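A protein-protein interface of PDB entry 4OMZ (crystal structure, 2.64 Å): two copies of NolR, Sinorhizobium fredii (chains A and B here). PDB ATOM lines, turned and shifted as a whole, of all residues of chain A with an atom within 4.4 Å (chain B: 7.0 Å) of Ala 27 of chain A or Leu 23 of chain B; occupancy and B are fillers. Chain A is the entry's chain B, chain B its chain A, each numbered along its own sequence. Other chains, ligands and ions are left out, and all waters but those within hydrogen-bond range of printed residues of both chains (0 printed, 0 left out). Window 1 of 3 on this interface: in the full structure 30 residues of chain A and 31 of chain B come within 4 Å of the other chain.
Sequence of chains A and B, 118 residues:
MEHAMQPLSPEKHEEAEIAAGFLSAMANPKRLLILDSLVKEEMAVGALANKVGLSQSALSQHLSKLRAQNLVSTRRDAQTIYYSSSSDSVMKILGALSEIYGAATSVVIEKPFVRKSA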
ATOM      1  N   LEU A  23     -28.292 -28.079   3.825  1.00  0.00           N
ATOM      2  CA  LEU A  23     -27.471 -27.690   4.965  1.00  0.00           C
ATOM      3  C   LEU A  23     -27.648 -28.677   6.105  1.00  0.00           C
ATOM      4  O   LEU A  23     -26.692 -28.981   6.822  1.00  0.00           O
ATOM      5  CB  LEU A  23     -27.822 -26.279   5.441  1.00  0.00           C
ATOM      6  CG  LEU A  23     -27.342 -25.105   4.594  1.00  0.00           C
ATOM      7  CD1 LEU A  23     -27.776 -23.801   5.233  1.00  0.00           C
ATOM      8  CD2 LEU A  23     -25.821 -25.148   4.446  1.00  0.00           C
ATOM      9  N   SER A  24     -28.866 -29.197   6.248  1.00  0.00           N
ATOM     10  CA  SER A  24     -29.154 -30.181   7.288  1.00  0.00           C
ATOM     11  C   SER A  24     -28.352 -31.442   7.060  1.00  0.00           C
ATOM     12  O   SER A  24     -27.839 -32.028   8.013  1.00  0.00           O
ATOM     13  CB  SER A  24     -30.644 -30.520   7.344  1.00  0.00           C
ATOM     14  OG  SER A  24     -31.367 -29.467   7.945  1.00  0.00           O
ATOM     15  N   ALA A  25     -28.226 -31.850   5.800  1.00  0.00           N
ATOM     16  CA  ALA A  25     -27.380 -33.003   5.506  1.00  0.00           C
ATOM     17  C   ALA A  25     -25.957 -32.716   5.962  1.00  0.00           C
ATOM     18  O   ALA A  25     -25.248 -33.617   6.427  1.00  0.00           O
ATOM     19  CB  ALA A  25     -27.400 -33.338   4.043  1.00  0.00           C
ATOM     20  N   MET A  26     -25.535 -31.459   5.834  1.00  0.00           N
ATOM     21  CA  MET A  26     -24.174 -31.118   6.272  1.00  0.00           C
ATOM     22  C   MET A  26     -24.031 -30.688   7.742  1.00  0.00           C
ATOM     23  O   MET A  26     -22.916 -30.682   8.275  1.00  0.00           O
ATOM     24  CB  MET A  26     -23.590 -30.026   5.379  1.00  0.00           C
ATOM     25  CG  MET A  26     -23.256 -30.498   3.981  1.00  0.00           C
ATOM     26  SD  MET A  26     -22.321 -29.259   3.074  1.00  0.00           S
ATOM     27  CE  MET A  26     -20.723 -29.383   3.886  1.00  0.00           C
ATOM     28  N   ALA A  27     -25.133 -30.315   8.393  1.00  0.00           N
ATOM     29  CA  ALA A  27     -25.048 -29.713   9.730  1.00  0.00           C
ATOM     30  C   ALA A  27     -24.913 -30.745  10.856  1.00  0.00           C
ATOM     31  O   ALA A  27     -25.675 -30.737  11.822  1.00  0.00           O
ATOM     32  CB  ALA A  27     -26.259 -28.824   9.980  1.00  0.00           C
ATOM     33  N   ASN A  28     -23.916 -31.611  10.729  1.00  0.00           N
ATOM     34  CA  ASN A  28     -23.586 -32.595  11.749  1.00  0.00           C
ATOM     35  C   ASN A  28     -22.069 -32.779  11.781  1.00  0.00           C
ATOM     36  O   ASN A  28     -21.434 -32.864  10.726  1.00  0.00           O
ATOM     37  CB  ASN A  28     -24.301 -33.923  11.466  1.00  0.00           C
ATOM     38  CG  ASN A  28     -23.956 -35.007  12.474  1.00  0.00           C
ATOM     39  OD1 ASN A  28     -22.987 -35.744  12.301  1.00  0.00           O
ATOM     40  ND2 ASN A  28     -24.758 -35.114  13.529  1.00  0.00           N
ATOM     41  N   LEU A  32     -19.663 -33.743   8.729  1.00  0.00           N
ATOM     42  CA  LEU A  32     -18.644 -32.824   8.248  1.00  0.00           C
ATOM     43  C   LEU A  32     -17.308 -33.546   8.115  1.00  0.00           C
ATOM     44  O   LEU A  32     -16.613 -33.381   7.117  1.00  0.00           O
ATOM     45  CB  LEU A  32     -18.497 -31.609   9.163  1.00  0.00           C
ATOM     46  CG  LEU A  32     -19.486 -30.469   8.895  1.00  0.00           C
ATOM     47  CD1 LEU A  32     -19.148 -29.245   9.748  1.00  0.00           C
ATOM     48  CD2 LEU A  32     -19.563 -30.113   7.405  1.00  0.00           C
ATOM     49  N   LEU A  97     -16.628 -22.606   5.068  1.00  0.00           N
ATOM     50  CA  LEU A  97     -16.250 -22.971   6.430  1.00  0.00           C
ATOM     51  C   LEU A  97     -14.746 -22.825   6.652  1.00  0.00           C
ATOM     52  O   LEU A  97     -14.300 -22.385   7.714  1.00  0.00           O
ATOM     53  CB  LEU A  97     -16.680 -24.408   6.734  1.00  0.00           C
ATOM     54  CG  LEU A  97     -18.174 -24.719   6.823  1.00  0.00           C
ATOM     55  CD1 LEU A  97     -18.384 -26.199   7.105  1.00  0.00           C
ATOM     56  CD2 LEU A  97     -18.845 -23.861   7.888  1.00  0.00           C
ATOM     57  N   ILE B  18     -17.809 -27.266  16.389  1.00  0.00           N
ATOM     58  CA  ILE B  18     -18.117 -25.834  16.300  1.00  0.00           C
ATOM     59  C   ILE B  18     -18.818 -25.464  14.980  1.00  0.00           C
ATOM     60  O   ILE B  18     -19.893 -24.819  14.969  1.00  0.00           O
ATOM     61  CB  ILE B  18     -16.846 -24.990  16.456  1.00  0.00           C
ATOM     62  CG1 ILE B  18     -16.316 -25.104  17.887  1.00  0.00           C
ATOM     63  CG2 ILE B  18     -17.119 -23.540  16.086  1.00  0.00           C
ATOM     64  CD1 ILE B  18     -14.861 -24.754  18.021  1.00  0.00           C
ATOM     65  N   ALA B  19     -18.216 -25.898  13.876  1.00  0.00           N
ATOM     66  CA  ALA B  19     -18.754 -25.631  12.549  1.00  0.00           C
ATOM     67  C   ALA B  19     -20.177 -26.169  12.425  1.00  0.00           C
ATOM     68  O   ALA B  19     -21.065 -25.495  11.896  1.00  0.00           O
ATOM     69  CB  ALA B  19     -17.860 -26.246  11.484  1.00  0.00           C
ATOM     70  N   ALA B  20     -20.393 -27.377  12.937  1.00  0.00           N
ATOM     71  CA  ALA B  20     -21.716 -27.986  12.874  1.00  0.00           C
ATOM     72  C   ALA B  20     -22.708 -27.231  13.753  1.00  0.00           C
ATOM     73  O   ALA B  20     -23.893 -27.207  13.450  1.00  0.00           O
ATOM     74  CB  ALA B  20     -21.657 -29.451  13.276  1.00  0.00           C
ATOM     75  N   GLY B  21     -22.236 -26.637  14.848  1.00  0.00           N
ATOM     76  CA  GLY B  21     -23.106 -25.808  15.675  1.00  0.00           C
ATOM     77  C   GLY B  21     -23.616 -24.600  14.901  1.00  0.00           C
ATOM     78  O   GLY B  21     -24.828 -24.313  14.857  1.00  0.00           O
ATOM     79  N   PHE B  22     -22.681 -23.907  14.257  1.00  0.00           N
ATOM     80  CA  PHE B  22     -23.022 -22.772  13.401  1.00  0.00           C
ATOM     81  C   PHE B  22     -23.999 -23.156  12.272  1.00  0.00           C
ATOM     82  O   PHE B  22     -25.075 -22.538  12.097  1.00  0.00           O
ATOM     83  CB  PHE B  22     -21.732 -22.192  12.830  1.00  0.00           C
ATOM     84  CG  PHE B  22     -21.921 -21.346  11.612  1.00  0.00           C
ATOM     85  CD1 PHE B  22     -22.622 -20.154  11.670  1.00  0.00           C
ATOM     86  CD2 PHE B  22     -21.380 -21.745  10.398  1.00  0.00           C
ATOM     87  CE1 PHE B  22     -22.779 -19.375  10.537  1.00  0.00           C
ATOM     88  CE2 PHE B  22     -21.535 -20.970   9.262  1.00  0.00           C
ATOM     89  CZ  PHE B  22     -22.236 -19.784   9.332  1.00  0.00           C
ATOM     90  N   LEU B  23     -23.640 -24.193  11.517  1.00  0.00           N
ATOM     91  CA  LEU B  23     -24.475 -24.643  10.405  1.00  0.00           C
ATOM     92  C   LEU B  23     -25.851 -25.059  10.903  1.00  0.00           C
ATOM     93  O   LEU B  23     -26.859 -24.856  10.228  1.00  0.00           O
ATOM     94  CB  LEU B  23     -23.839 -25.818   9.673  1.00  0.00           C
ATOM     95  CG  LEU B  23     -22.611 -25.534   8.824  1.00  0.00           C
ATOM     96  CD1 LEU B  23     -22.130 -26.824   8.189  1.00  0.00           C
ATOM     97  CD2 LEU B  23     -22.964 -24.497   7.783  1.00  0.00           C
ATOM     98  N   SER B  24     -25.877 -25.638  12.097  1.00  0.00           N
ATOM     99  CA  SER B  24     -27.122 -26.064  12.711  1.00  0.00           C
ATOM    100  C   SER B  24     -27.990 -24.850  12.961  1.00  0.00           C
ATOM    101  O   SER B  24     -29.207 -24.914  12.791  1.00  0.00           O
ATOM    102  CB  SER B  24     -26.864 -26.808  14.019  1.00  0.00           C
ATOM    103  OG  SER B  24     -26.338 -28.097  13.760  1.00  0.00           O
ATOM    104  N   ALA B  25     -27.365 -23.748  13.376  1.00  0.00           N
ATOM    105  CA  ALA B  25     -28.114 -22.503  13.529  1.00  0.00           C
ATOM    106  C   ALA B  25     -28.698 -22.069  12.194  1.00  0.00           C
ATOM    107  O   ALA B  25     -29.792 -21.508  12.146  1.00  0.00           O
ATOM    108  CB  ALA B  25     -27.246 -21.406  14.096  1.00  0.00           C
ATOM    109  N   MET B  26     -27.974 -22.311  11.106  1.00  0.00           N
ATOM    110  CA  MET B  26     -28.511 -21.898   9.806  1.00  0.00           C
ATOM    111  C   MET B  26     -29.371 -22.945   9.086  1.00  0.00           C
ATOM    112  O   MET B  26     -30.162 -22.591   8.215  1.00  0.00           O
ATOM    113  CB  MET B  26     -27.377 -21.481   8.875  1.00  0.00           C
ATOM    114  CG  MET B  26     -26.693 -20.202   9.290  1.00  0.00           C
ATOM    115  SD  MET B  26     -25.591 -19.610   8.003  1.00  0.00           S
ATOM    116  CE  MET B  26     -26.784 -18.976   6.817  1.00  0.00           C
ATOM    117  N   ALA B  27     -29.242 -24.217   9.452  1.00  0.00           N
ATOM    118  CA  ALA B  27     -29.881 -25.286   8.679  1.00  0.00           C
ATOM    119  C   ALA B  27     -31.355 -25.456   9.043  1.00  0.00           C
ATOM    120  O   ALA B  27     -31.798 -26.545   9.408  1.00  0.00           O
ATOM    121  CB  ALA B  27     -29.138 -26.602   8.867  1.00  0.00           C
ATOM    122  N   ASN B  28     -32.102 -24.364   8.947  1.00  0.00           N
ATOM    123  CA  ASN B  28     -33.543 -24.383   9.146  1.00  0.00           C
ATOM    124  C   ASN B  28     -34.171 -23.375   8.191  1.00  0.00           C
ATOM    125  O   ASN B  28     -33.664 -22.260   8.055  1.00  0.00           O
ATOM    126  CB  ASN B  28     -33.885 -24.060  10.600  1.00  0.00           C
ATOM    127  CG  ASN B  28     -35.378 -24.047  10.862  1.00  0.00           C
ATOM    128  OD1 ASN B  28     -36.046 -23.019  10.717  1.00  0.00           O
ATOM    129  ND2 ASN B  28     -35.910 -25.194  11.264  1.00  0.00           N
ATOM    130  N   ARG B  31     -35.298 -20.077   9.802  1.00  0.00           N
ATOM    131  CA  ARG B  31     -34.091 -19.350  10.198  1.00  0.00           C
ATOM    132  C   ARG B  31     -33.331 -18.788   9.000  1.00  0.00           C
ATOM    133  O   ARG B  31     -32.727 -17.721   9.084  1.00  0.00           O
ATOM    134  CB  ARG B  31     -33.169 -20.256  11.007  1.00  0.00           C
ATOM    135  CG  ARG B  31     -32.986 -19.813  12.437  1.00  0.00           C
ATOM    136  CD  ARG B  31     -33.327 -20.922  13.396  1.00  0.00           C
ATOM    137  NE  ARG B  31     -32.483 -22.101  13.248  1.00  0.00           N
ATOM    138  CZ  ARG B  31     -32.837 -23.308  13.678  1.00  0.00           C
ATOM    139  NH1 ARG B  31     -34.016 -23.480  14.264  1.00  0.00           N
ATOM    140  NH2 ARG B  31     -32.027 -24.340  13.512  1.00  0.00           N
ATOM    141  N   LYS B  65     -32.104 -19.123  19.102  1.00  0.00           N
ATOM    142  CA  LYS B  65     -31.040 -20.045  18.658  1.00  0.00           C
ATOM    143  C   LYS B  65     -29.976 -19.307  17.814  1.00  0.00           C
ATOM    144  O   LYS B  65     -28.783 -19.650  17.845  1.00  0.00           O
ATOM    145  CB  LYS B  65     -31.619 -21.233  17.892  1.00  0.00           C
ATOM    146  CG  LYS B  65     -30.591 -21.946  17.013  1.00  0.00           C
ATOM    147  CD  LYS B  65     -30.462 -23.427  17.376  1.00  0.00           C
ATOM    148  CE  LYS B  65     -29.215 -24.070  16.771  1.00  0.00           C
ATOM    149  NZ  LYS B  65     -29.366 -25.541  16.586  1.00  0.00           N
ATOM    150  N   GLN B  69     -25.661 -18.573  18.563  1.00  0.00           N
ATOM    151  CA  GLN B  69     -24.516 -18.685  17.667  1.00  0.00           C
ATOM    152  C   GLN B  69     -23.976 -17.318  17.269  1.00  0.00           C
ATOM    153  O   GLN B  69     -23.201 -17.215  16.321  1.00  0.00           O
ATOM    154  CB  GLN B  69     -24.893 -19.475  16.415  1.00  0.00           C
ATOM    155  CG  GLN B  69     -24.977 -20.973  16.622  1.00  0.00           C
ATOM    156  CD  GLN B  69     -23.634 -21.592  16.923  1.00  0.00           C
ATOM    157  OE1 GLN B  69     -22.605 -21.146  16.415  1.00  0.00           O
ATOM    158  NE2 GLN B  69     -23.635 -22.637  17.739  1.00  0.00           N
ATOM    159  N   LEU B  71     -25.178 -14.721  15.795  1.00  0.00           N
ATOM    160  CA  LEU B  71     -25.408 -14.433  14.384  1.00  0.00           C
ATOM    161  C   LEU B  71     -26.238 -13.176  14.150  1.00  0.00           C
ATOM    162  O   LEU B  71     -26.416 -12.752  13.006  1.00  0.00           O
ATOM    163  CB  LEU B  71     -26.086 -15.625  13.707  1.00  0.00           C
ATOM    164  CG  LEU B  71     -25.304 -16.940  13.757  1.00  0.00           C
ATOM    165  CD1 LEU B  71     -26.057 -18.043  13.047  1.00  0.00           C
ATOM    166  CD2 LEU B  71     -23.921 -16.759  13.155  1.00  0.00           C
ATOM    167  N   ILE B  93     -22.058 -18.060   4.026  1.00  0.00           N
ATOM    168  CA  ILE B  93     -22.905 -19.214   3.735  1.00  0.00           C
ATOM    169  C   ILE B  93     -24.016 -18.834   2.754  1.00  0.00           C
ATOM    170  O   ILE B  93     -24.291 -19.578   1.816  1.00  0.00           O
ATOM    171  CB  ILE B  93     -23.511 -19.820   5.009  1.00  0.00           C
ATOM    172  CG1 ILE B  93     -22.395 -20.379   5.896  1.00  0.00           C
ATOM    173  CG2 ILE B  93     -24.489 -20.931   4.659  1.00  0.00           C
ATOM    174  CD1 ILE B  93     -21.529 -21.405   5.208  1.00  0.00           C
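Leu 23 of chain A touches Ala 27 of chain B, and with the chains exchanged Ala 27 of chain A touches Leu 23 of chain B. Ser 24 of chain A touches Ala 27 of chain B, and with the chains exchanged Ala 27 of chain A touches Ser 24 of chain B. Met 26 of chain A touches Leu 23 of chain B, but with the chains exchanged Leu 23 of chain A does not touch Met 26 of chain B (4.01 Å). Ala 27 of chain B touches its own counterpart, Ala 27 of chain A. Of the 10 pairs that touch across the chains among the printed residues, 5 have their exchanged pair printed and touching as well.
Of the 8 printed residues of chain A, 7 touch a printed residue of chain B. Hydrophobic or aromatic side chains of chain A within 4 Å of the printed part of chain B: Leu 23, Ala 27, Leu 32 and Leu 97. Printed residues of chain B that touch a printed residue of chain A: Ala 19, Ala 20, Leu 23, Ser 24 and Ala 27. Hydrophobic or aromatic side chains of chain B within 4 Å of the printed part of chain A: Ala 19, Ala 20, Leu 23 and Ala 27.
The backbone carbonyl oxygen (O) of Ala 27 of chain A is in hydrogen-bond range of the side-chain hydroxyl (OG) of Ser 24 of chain B, 3.3 Å away. The backbone carbonyl oxygen (O) of Ala 27 of chain B lies within hydrogen-bond range of the side-chain hydroxyl (OG) of Ser 24 of chain A (3.3 Å).
Among the printed residues, pairs that only touch across the chains: Asn 28 of chain A with Ala 20 of chain B (3.7 Å), Leu 23 of chain A with Ala 27 of chain B (3.7 Å), Leu 32 of chain A with Ala 19 of chain B (3.7 Å), Ala 27 of chain A with Ala 27 of chain B (3.8 Å), Ala 27 of chain A with Leu 23 of chain B (3.9 Å), Leu 32 of chain A with Ala 20 of chain B (3.9 Å), Met 26 of chain A with Leu 23 of chain B (3.9 Å) and Leu 97 of chain A with Leu 23 of chain B (3.9 Å).
OG of Ser 24 of chain B is in hydrogen-bond range of O of Ala 20 of chain B (2.6 Å). The guanidinium group (NH2) of Arg 31 of chain B is in hydrogen-bond range of the backbone carbonyl oxygen (O) of Ser 24 of chain B, 3.0 Å away.
Of chain B, only Leu 23, Ser 24 and Ala 27 come within 4 Å of Ala 27 of chain A. Leu 23 of chain B touches three residues of chain A. Of the printed residues of chain A, Ser 24 of chain B touches Ala 27 (3.3 Å). Printed residues of chain B within 4 Å of Asn 28 of chain A: Ala 20 (3.7 Å). Leu 71 of chain B touches none of the printed residues of chain A. The nearest residue of chain B that does not touch Ala 27 of chain A is Ala 20 of chain B (4.3 Å). The nearest printed residue of chain B that does not touch Leu 97 of chain A is Phe 22 of chain B (4.1 Å).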
